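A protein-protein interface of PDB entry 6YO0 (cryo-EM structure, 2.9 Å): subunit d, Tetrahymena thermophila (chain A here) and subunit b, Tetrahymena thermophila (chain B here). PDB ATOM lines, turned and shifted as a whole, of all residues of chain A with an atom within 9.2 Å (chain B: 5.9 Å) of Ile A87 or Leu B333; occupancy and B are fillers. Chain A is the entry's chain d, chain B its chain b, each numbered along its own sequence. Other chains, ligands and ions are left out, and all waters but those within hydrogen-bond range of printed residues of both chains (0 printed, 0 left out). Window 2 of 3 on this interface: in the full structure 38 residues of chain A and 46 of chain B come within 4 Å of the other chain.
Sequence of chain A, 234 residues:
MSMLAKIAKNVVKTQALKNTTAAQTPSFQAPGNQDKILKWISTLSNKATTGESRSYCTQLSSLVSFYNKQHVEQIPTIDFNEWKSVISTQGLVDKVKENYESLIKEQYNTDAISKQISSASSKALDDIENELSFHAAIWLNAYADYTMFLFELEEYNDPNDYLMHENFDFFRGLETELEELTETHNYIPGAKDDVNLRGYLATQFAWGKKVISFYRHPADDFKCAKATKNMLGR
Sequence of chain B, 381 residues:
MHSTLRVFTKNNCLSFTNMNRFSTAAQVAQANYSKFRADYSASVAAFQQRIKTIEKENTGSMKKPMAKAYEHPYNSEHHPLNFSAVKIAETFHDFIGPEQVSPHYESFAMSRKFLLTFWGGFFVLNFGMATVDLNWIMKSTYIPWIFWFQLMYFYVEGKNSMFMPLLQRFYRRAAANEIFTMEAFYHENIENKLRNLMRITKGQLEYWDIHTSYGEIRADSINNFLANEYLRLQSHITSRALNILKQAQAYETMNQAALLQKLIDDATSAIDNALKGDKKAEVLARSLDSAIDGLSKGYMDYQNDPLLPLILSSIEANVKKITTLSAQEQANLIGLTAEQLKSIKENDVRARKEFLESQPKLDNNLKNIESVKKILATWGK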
ATOM      1  N   PHE A  80     -23.592   7.352  15.536  1.00  0.00           N
ATOM      2  CA  PHE A  80     -23.519   6.135  14.734  1.00  0.00           C
ATOM      3  C   PHE A  80     -24.068   6.353  13.331  1.00  0.00           C
ATOM      4  O   PHE A  80     -23.597   5.727  12.376  1.00  0.00           O
ATOM      5  CB  PHE A  80     -24.285   5.013  15.429  1.00  0.00           C
ATOM      6  CG  PHE A  80     -23.610   4.499  16.661  1.00  0.00           C
ATOM      7  CD1 PHE A  80     -22.535   3.636  16.568  1.00  0.00           C
ATOM      8  CD2 PHE A  80     -24.052   4.879  17.914  1.00  0.00           C
ATOM      9  CE1 PHE A  80     -21.913   3.163  17.703  1.00  0.00           C
ATOM     10  CE2 PHE A  80     -23.433   4.409  19.051  1.00  0.00           C
ATOM     11  CZ  PHE A  80     -22.362   3.551  18.945  1.00  0.00           C
ATOM     12  N   ASN A  81     -25.056   7.236  13.186  1.00  0.00           N
ATOM     13  CA  ASN A  81     -25.608   7.512  11.865  1.00  0.00           C
ATOM     14  C   ASN A  81     -24.555   8.106  10.941  1.00  0.00           C
ATOM     15  O   ASN A  81     -24.468   7.730   9.766  1.00  0.00           O
ATOM     16  CB  ASN A  81     -26.807   8.450  11.987  1.00  0.00           C
ATOM     17  CG  ASN A  81     -27.970   7.813  12.719  1.00  0.00           C
ATOM     18  OD1 ASN A  81     -28.140   6.593  12.695  1.00  0.00           O
ATOM     19  ND2 ASN A  81     -28.778   8.636  13.375  1.00  0.00           N
ATOM     20  N   GLU A  82     -23.744   9.034  11.452  1.00  0.00           N
ATOM     21  CA  GLU A  82     -22.705   9.629  10.619  1.00  0.00           C
ATOM     22  C   GLU A  82     -21.755   8.565  10.094  1.00  0.00           C
ATOM     23  O   GLU A  82     -21.387   8.577   8.914  1.00  0.00           O
ATOM     24  CB  GLU A  82     -21.943  10.689  11.413  1.00  0.00           C
ATOM     25  CG  GLU A  82     -20.868  11.415  10.620  1.00  0.00           C
ATOM     26  CD  GLU A  82     -19.553  10.657  10.566  1.00  0.00           C
ATOM     27  OE1 GLU A  82     -19.416   9.639  11.277  1.00  0.00           O
ATOM     28  OE2 GLU A  82     -18.654  11.079   9.810  1.00  0.00           O
ATOM     29  N   TRP A  83     -21.351   7.631  10.953  1.00  0.00           N
ATOM     30  CA  TRP A  83     -20.463   6.565  10.511  1.00  0.00           C
ATOM     31  C   TRP A  83     -21.170   5.655   9.518  1.00  0.00           C
ATOM     32  O   TRP A  83     -20.631   5.331   8.454  1.00  0.00           O
ATOM     33  CB  TRP A  83     -19.984   5.763  11.718  1.00  0.00           C
ATOM     34  CG  TRP A  83     -19.247   6.573  12.733  1.00  0.00           C
ATOM     35  CD1 TRP A  83     -19.648   6.851  14.006  1.00  0.00           C
ATOM     36  CD2 TRP A  83     -17.970   7.201  12.569  1.00  0.00           C
ATOM     37  NE1 TRP A  83     -18.703   7.614  14.645  1.00  0.00           N
ATOM     38  CE2 TRP A  83     -17.663   7.843  13.784  1.00  0.00           C
ATOM     39  CE3 TRP A  83     -17.057   7.281  11.515  1.00  0.00           C
ATOM     40  CZ2 TRP A  83     -16.485   8.559  13.972  1.00  0.00           C
ATOM     41  CZ3 TRP A  83     -15.890   7.993  11.704  1.00  0.00           C
ATOM     42  CH2 TRP A  83     -15.614   8.622  12.922  1.00  0.00           C
ATOM     43  N   LYS A  84     -22.386   5.232   9.862  1.00  0.00           N
ATOM     44  CA  LYS A  84     -23.189   4.414   8.962  1.00  0.00           C
ATOM     45  C   LYS A  84     -23.362   5.092   7.609  1.00  0.00           C
ATOM     46  O   LYS A  84     -23.398   4.425   6.569  1.00  0.00           O
ATOM     47  CB  LYS A  84     -24.543   4.146   9.615  1.00  0.00           C
ATOM     48  CG  LYS A  84     -25.582   3.460   8.748  1.00  0.00           C
ATOM     49  CD  LYS A  84     -26.985   3.892   9.158  1.00  0.00           C
ATOM     50  CE  LYS A  84     -27.233   3.706  10.653  1.00  0.00           C
ATOM     51  NZ  LYS A  84     -28.594   4.159  11.051  1.00  0.00           N
ATOM     52  N   SER A  85     -23.470   6.420   7.605  1.00  0.00           N
ATOM     53  CA  SER A  85     -23.722   7.152   6.369  1.00  0.00           C
ATOM     54  C   SER A  85     -22.451   7.325   5.548  1.00  0.00           C
ATOM     55  O   SER A  85     -22.421   6.979   4.363  1.00  0.00           O
ATOM     56  CB  SER A  85     -24.336   8.516   6.684  1.00  0.00           C
ATOM     57  OG  SER A  85     -23.453   9.300   7.464  1.00  0.00           O
ATOM     58  N   VAL A  86     -21.397   7.865   6.156  1.00  0.00           N
ATOM     59  CA  VAL A  86     -20.190   8.213   5.414  1.00  0.00           C
ATOM     60  C   VAL A  86     -19.686   6.970   4.694  1.00  0.00           C
ATOM     61  O   VAL A  86     -19.695   6.912   3.460  1.00  0.00           O
ATOM     62  CB  VAL A  86     -19.102   8.814   6.331  1.00  0.00           C
ATOM     63  CG1 VAL A  86     -18.887   7.976   7.593  1.00  0.00           C
ATOM     64  CG2 VAL A  86     -17.792   8.976   5.566  1.00  0.00           C
ATOM     65  N   ILE A  87     -19.245   5.966   5.449  1.00  0.00           N
ATOM     66  CA  ILE A  87     -18.767   4.728   4.851  1.00  0.00           C
ATOM     67  C   ILE A  87     -18.629   3.682   5.947  1.00  0.00           C
ATOM     68  O   ILE A  87     -18.241   4.001   7.076  1.00  0.00           O
ATOM     69  CB  ILE A  87     -17.433   4.949   4.115  1.00  0.00           C
ATOM     70  CG1 ILE A  87     -16.951   3.653   3.460  1.00  0.00           C
ATOM     71  CG2 ILE A  87     -16.373   5.465   5.078  1.00  0.00           C
ATOM     72  CD1 ILE A  87     -17.956   3.019   2.513  1.00  0.00           C
ATOM     73  N   SER A  88     -18.941   2.431   5.625  1.00  0.00           N
ATOM     74  CA  SER A  88     -18.721   1.322   6.543  1.00  0.00           C
ATOM     75  C   SER A  88     -19.166   0.040   5.855  1.00  0.00           C
ATOM     76  O   SER A  88     -19.870   0.074   4.842  1.00  0.00           O
ATOM     77  CB  SER A  88     -19.472   1.513   7.861  1.00  0.00           C
ATOM     78  OG  SER A  88     -18.967   2.628   8.576  1.00  0.00           O
ATOM     79  N   THR A  89     -18.742  -1.089   6.415  1.00  0.00           N
ATOM     80  CA  THR A  89     -19.225  -2.377   5.943  1.00  0.00           C
ATOM     81  C   THR A  89     -20.653  -2.616   6.418  1.00  0.00           C
ATOM     82  O   THR A  89     -20.992  -2.370   7.578  1.00  0.00           O
ATOM     83  CB  THR A  89     -18.317  -3.502   6.435  1.00  0.00           C
ATOM     84  OG1 THR A  89     -16.989  -3.302   5.939  1.00  0.00           O
ATOM     85  CG2 THR A  89     -18.833  -4.847   5.954  1.00  0.00           C
ATOM     86  N   GLN A  90     -21.490  -3.099   5.505  1.00  0.00           N
ATOM     87  CA  GLN A  90     -22.898  -3.334   5.793  1.00  0.00           C
ATOM     88  C   GLN A  90     -23.070  -4.223   7.017  1.00  0.00           C
ATOM     89  O   GLN A  90     -22.548  -5.341   7.063  1.00  0.00           O
ATOM     90  CB  GLN A  90     -23.573  -3.967   4.576  1.00  0.00           C
ATOM     91  CG  GLN A  90     -22.974  -5.299   4.154  1.00  0.00           C
ATOM     92  CD  GLN A  90     -23.690  -6.488   4.766  1.00  0.00           C
ATOM     93  OE1 GLN A  90     -24.588  -6.330   5.592  1.00  0.00           O
ATOM     94  NE2 GLN A  90     -23.290  -7.687   4.365  1.00  0.00           N
ATOM     95  N   LEU A  92     -21.859  -3.679  10.016  1.00  0.00           N
ATOM     96  CA  LEU A  92     -20.819  -3.507  11.022  1.00  0.00           C
ATOM     97  C   LEU A  92     -21.169  -2.376  11.977  1.00  0.00           C
ATOM     98  O   LEU A  92     -21.088  -2.536  13.199  1.00  0.00           O
ATOM     99  CB  LEU A  92     -19.479  -3.248  10.334  1.00  0.00           C
ATOM    100  CG  LEU A  92     -18.235  -3.137  11.216  1.00  0.00           C
ATOM    101  CD1 LEU A  92     -16.995  -3.386  10.385  1.00  0.00           C
ATOM    102  CD2 LEU A  92     -18.152  -1.782  11.889  1.00  0.00           C
ATOM    103  N   VAL A  93     -21.567  -1.225  11.434  1.00  0.00           N
ATOM    104  CA  VAL A  93     -21.863  -0.071  12.276  1.00  0.00           C
ATOM    105  C   VAL A  93     -23.022  -0.388  13.209  1.00  0.00           C
ATOM    106  O   VAL A  93     -22.981  -0.074  14.405  1.00  0.00           O
ATOM    107  CB  VAL A  93     -22.156   1.167  11.406  1.00  0.00           C
ATOM    108  CG1 VAL A  93     -23.345   0.917  10.486  1.00  0.00           C
ATOM    109  CG2 VAL A  93     -22.396   2.385  12.280  1.00  0.00           C
ATOM    110  N   LEU B 245     -14.179   1.629  15.019  1.00  0.00           N
ATOM    111  CA  LEU B 245     -14.797   2.141  13.806  1.00  0.00           C
ATOM    112  C   LEU B 245     -13.826   3.002  13.010  1.00  0.00           C
ATOM    113  O   LEU B 245     -13.770   2.906  11.779  1.00  0.00           O
ATOM    114  CB  LEU B 245     -16.045   2.932  14.181  1.00  0.00           C
ATOM    115  CG  LEU B 245     -17.107   3.113  13.108  1.00  0.00           C
ATOM    116  CD1 LEU B 245     -18.379   3.595  13.761  1.00  0.00           C
ATOM    117  CD2 LEU B 245     -16.631   4.089  12.056  1.00  0.00           C
ATOM    118  N   GLN B 249     -12.421   2.306   9.193  1.00  0.00           N
ATOM    119  CA  GLN B 249     -12.479   3.281   8.111  1.00  0.00           C
ATOM    120  C   GLN B 249     -11.120   3.452   7.452  1.00  0.00           C
ATOM    121  O   GLN B 249     -11.025   3.546   6.222  1.00  0.00           O
ATOM    122  CB  GLN B 249     -12.996   4.615   8.645  1.00  0.00           C
ATOM    123  CG  GLN B 249     -12.930   5.762   7.658  1.00  0.00           C
ATOM    124  CD  GLN B 249     -13.358   7.076   8.278  1.00  0.00           C
ATOM    125  OE1 GLN B 249     -13.900   7.106   9.382  1.00  0.00           O
ATOM    126  NE2 GLN B 249     -13.121   8.171   7.566  1.00  0.00           N
ATOM    127  N   GLU B 252     -10.540   0.629   5.173  1.00  0.00           N
ATOM    128  CA  GLU B 252     -11.374   0.735   3.980  1.00  0.00           C
ATOM    129  C   GLU B 252     -10.787   1.711   2.972  1.00  0.00           C
ATOM    130  O   GLU B 252     -10.762   1.430   1.768  1.00  0.00           O
ATOM    131  CB  GLU B 252     -12.788   1.162   4.373  1.00  0.00           C
ATOM    132  CG  GLU B 252     -13.478   0.202   5.328  1.00  0.00           C
ATOM    133  CD  GLU B 252     -14.957   0.486   5.497  1.00  0.00           C
ATOM    134  OE1 GLU B 252     -15.534   1.182   4.639  1.00  0.00           O
ATOM    135  OE2 GLU B 252     -15.547   0.005   6.486  1.00  0.00           O
ATOM    136  N   ASN B 255      -8.015   0.003   1.259  1.00  0.00           N
ATOM    137  CA  ASN B 255      -8.504  -0.959   0.279  1.00  0.00           C
ATOM    138  C   ASN B 255      -8.909  -0.263  -1.013  1.00  0.00           C
ATOM    139  O   ASN B 255      -8.532  -0.694  -2.109  1.00  0.00           O
ATOM    140  CB  ASN B 255      -9.688  -1.732   0.859  1.00  0.00           C
ATOM    141  CG  ASN B 255      -9.269  -2.778   1.867  1.00  0.00           C
ATOM    142  OD1 ASN B 255      -9.264  -2.532   3.072  1.00  0.00           O
ATOM    143  ND2 ASN B 255      -8.921  -3.961   1.376  1.00  0.00           N
ATOM    144  N   GLN B 256      -9.677   0.821  -0.903  1.00  0.00           N
ATOM    145  CA  GLN B 256     -10.091   1.554  -2.093  1.00  0.00           C
ATOM    146  C   GLN B 256      -8.891   2.106  -2.850  1.00  0.00           C
ATOM    147  O   GLN B 256      -8.827   2.018  -4.081  1.00  0.00           O
ATOM    148  CB  GLN B 256     -11.033   2.686  -1.692  1.00  0.00           C
ATOM    149  CG  GLN B 256     -11.550   3.518  -2.849  1.00  0.00           C
ATOM    150  CD  GLN B 256     -12.551   4.568  -2.405  1.00  0.00           C
ATOM    151  OE1 GLN B 256     -13.001   4.568  -1.260  1.00  0.00           O
ATOM    152  NE2 GLN B 256     -12.902   5.470  -3.312  1.00  0.00           N
ATOM    153  N   LEU B 259      -7.135  -0.607  -4.833  1.00  0.00           N
ATOM    154  CA  LEU B 259      -7.856  -0.967  -6.046  1.00  0.00           C
ATOM    155  C   LEU B 259      -7.583   0.029  -7.165  1.00  0.00           C
ATOM    156  O   LEU B 259      -7.303  -0.359  -8.305  1.00  0.00           O
ATOM    157  CB  LEU B 259      -9.352  -1.039  -5.751  1.00  0.00           C
ATOM    158  CG  LEU B 259     -10.246  -1.389  -6.935  1.00  0.00           C
ATOM    159  CD1 LEU B 259      -9.845  -2.728  -7.522  1.00  0.00           C
ATOM    160  CD2 LEU B 259     -11.699  -1.394  -6.507  1.00  0.00           C
ATOM    161  N   GLN B 328     -22.684  -5.028  -4.910  1.00  0.00           N
ATOM    162  CA  GLN B 328     -21.371  -5.655  -5.009  1.00  0.00           C
ATOM    163  C   GLN B 328     -20.286  -4.693  -4.553  1.00  0.00           C
ATOM    164  O   GLN B 328     -19.291  -5.107  -3.947  1.00  0.00           O
ATOM    165  CB  GLN B 328     -21.096  -6.122  -6.441  1.00  0.00           C
ATOM    166  CG  GLN B 328     -22.134  -7.072  -7.021  1.00  0.00           C
ATOM    167  CD  GLN B 328     -23.348  -6.353  -7.572  1.00  0.00           C
ATOM    168  OE1 GLN B 328     -23.292  -5.162  -7.872  1.00  0.00           O
ATOM    169  NE2 GLN B 328     -24.454  -7.074  -7.705  1.00  0.00           N
ATOM    170  N   GLU B 329     -20.462  -3.402  -4.836  1.00  0.00           N
ATOM    171  CA  GLU B 329     -19.498  -2.413  -4.375  1.00  0.00           C
ATOM    172  C   GLU B 329     -19.353  -2.443  -2.862  1.00  0.00           C
ATOM    173  O   GLU B 329     -18.277  -2.135  -2.339  1.00  0.00           O
ATOM    174  CB  GLU B 329     -19.918  -1.021  -4.845  1.00  0.00           C
ATOM    175  CG  GLU B 329     -19.886  -0.855  -6.351  1.00  0.00           C
ATOM    176  CD  GLU B 329     -20.366   0.510  -6.796  1.00  0.00           C
ATOM    177  OE1 GLU B 329     -20.545   1.388  -5.927  1.00  0.00           O
ATOM    178  OE2 GLU B 329     -20.565   0.707  -8.013  1.00  0.00           O
ATOM    179  N   GLN B 330     -20.419  -2.805  -2.141  1.00  0.00           N
ATOM    180  CA  GLN B 330     -20.325  -2.906  -0.689  1.00  0.00           C
ATOM    181  C   GLN B 330     -19.097  -3.706  -0.276  1.00  0.00           C
ATOM    182  O   GLN B 330     -18.360  -3.310   0.632  1.00  0.00           O
ATOM    183  CB  GLN B 330     -21.589  -3.549  -0.113  1.00  0.00           C
ATOM    184  CG  GLN B 330     -22.882  -2.835  -0.459  1.00  0.00           C
ATOM    185  CD  GLN B 330     -24.107  -3.619  -0.037  1.00  0.00           C
ATOM    186  OE1 GLN B 330     -24.000  -4.732   0.474  1.00  0.00           O
ATOM    187  NE2 GLN B 330     -25.281  -3.037  -0.247  1.00  0.00           N
ATOM    188  N   ALA B 331     -18.870  -4.844  -0.928  1.00  0.00           N
ATOM    189  CA  ALA B 331     -17.703  -5.662  -0.627  1.00  0.00           C
ATOM    190  C   ALA B 331     -16.536  -5.365  -1.557  1.00  0.00           C
ATOM    191  O   ALA B 331     -15.377  -5.403  -1.130  1.00  0.00           O
ATOM    192  CB  ALA B 331     -18.068  -7.145  -0.715  1.00  0.00           C
ATOM    193  N   ASN B 332     -16.822  -5.071  -2.826  1.00  0.00           N
ATOM    194  CA  ASN B 332     -15.756  -4.783  -3.778  1.00  0.00           C
ATOM    195  C   ASN B 332     -14.925  -3.593  -3.324  1.00  0.00           C
ATOM    196  O   ASN B 332     -13.689  -3.650  -3.309  1.00  0.00           O
ATOM    197  CB  ASN B 332     -16.348  -4.528  -5.164  1.00  0.00           C
ATOM    198  CG  ASN B 332     -15.287  -4.325  -6.235  1.00  0.00           C
ATOM    199  OD1 ASN B 332     -15.560  -3.725  -7.274  1.00  0.00           O
ATOM    200  ND2 ASN B 332     -14.080  -4.830  -5.997  1.00  0.00           N
ATOM    201  N   LEU B 333     -15.590  -2.502  -2.946  1.00  0.00           N
ATOM    202  CA  LEU B 333     -14.870  -1.324  -2.476  1.00  0.00           C
ATOM    203  C   LEU B 333     -14.072  -1.646  -1.220  1.00  0.00           C
ATOM    204  O   LEU B 333     -12.888  -1.307  -1.117  1.00  0.00           O
ATOM    205  CB  LEU B 333     -15.855  -0.179  -2.222  1.00  0.00           C
ATOM    206  CG  LEU B 333     -15.424   0.970  -1.304  1.00  0.00           C
ATOM    207  CD1 LEU B 333     -14.305   1.787  -1.925  1.00  0.00           C
ATOM    208  CD2 LEU B 333     -16.609   1.862  -0.961  1.00  0.00           C
ATOM    209  N   ILE B 334     -14.704  -2.300  -0.254  1.00  0.00           N
ATOM    210  CA  ILE B 334     -14.083  -2.597   1.034  1.00  0.00           C
ATOM    211  C   ILE B 334     -14.095  -4.113   1.205  1.00  0.00           C
ATOM    212  O   ILE B 334     -15.023  -4.702   1.764  1.00  0.00           O
ATOM    213  CB  ILE B 334     -14.783  -1.876   2.190  1.00  0.00           C
ATOM    214  CG1 ILE B 334     -16.270  -2.237   2.270  1.00  0.00           C
ATOM    215  CG2 ILE B 334     -14.684  -0.392   1.998  1.00  0.00           C
ATOM    216  CD1 ILE B 334     -17.032  -1.492   3.353  1.00  0.00           C
ATOM    217  N   GLY B 335     -13.044  -4.765   0.717  1.00  0.00           N
ATOM    218  CA  GLY B 335     -12.906  -6.198   0.874  1.00  0.00           C
ATOM    219  C   GLY B 335     -12.175  -6.559   2.150  1.00  0.00           C
ATOM    220  O   GLY B 335     -11.080  -7.128   2.094  1.00  0.00           O
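The backbone NH of Thr A89 lies within hydrogen-bond range of the side-chain carboxylate of Glu B252, at 3.4 Å.
O of Trp A83 sits at hydrogen-bond distance from OG of Ser A88 (3.2 Å).
Among the printed residues, pairs that only touch across the chains: Trp A83 with Leu B245, Trp A83 with Gln B249, Ile A87 with Glu B252, Ile A87 with Leu B333, Ser A88 with Glu B252, Ser A88 with Ile B334, Thr A89 with Ile B334 and Gln A90 with Gln B330.
Ile A87 touches just these residues of chain B: Glu B252 (3.1 Å) and Leu B333 (3.9 Å).
Leu B333 touches one residue of chain A.
Asn B332 touches none of the printed residues of chain A.
Ile B334 touches two residues of chain A.
Printed residues of chain B within 4 Å of Thr A89: Glu B252 (3.4 Å) and Ile B334 (3.2 Å).
Of the printed residues of chain A, Gln B249 touches Trp A83 (3.2 Å).
The nearest residue of chain B that does not touch Ile A87 is Gln B249 (4.3 Å).
The nearest residue of chain A that does not touch Leu B333 is Ser A88 (6.9 Å).
The nearest printed residue of chain B that does not touch Trp A83 is Glu B252 (7.6 Å).
Printed residues of chain A that touch a printed residue of chain B: Trp A83, Ile A87, Ser A88, Thr A89 and Gln A90.
Hydrophobic or aromatic side chains of chain A within 4 Å of the printed part of chain B: Trp A83 and Ile A87.
Along chain A the printed residues that touch a printed residue of chain B span positions 83 to 90.
Along chain B the printed residues that touch a printed residue of chain A span positions 245 to 334.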
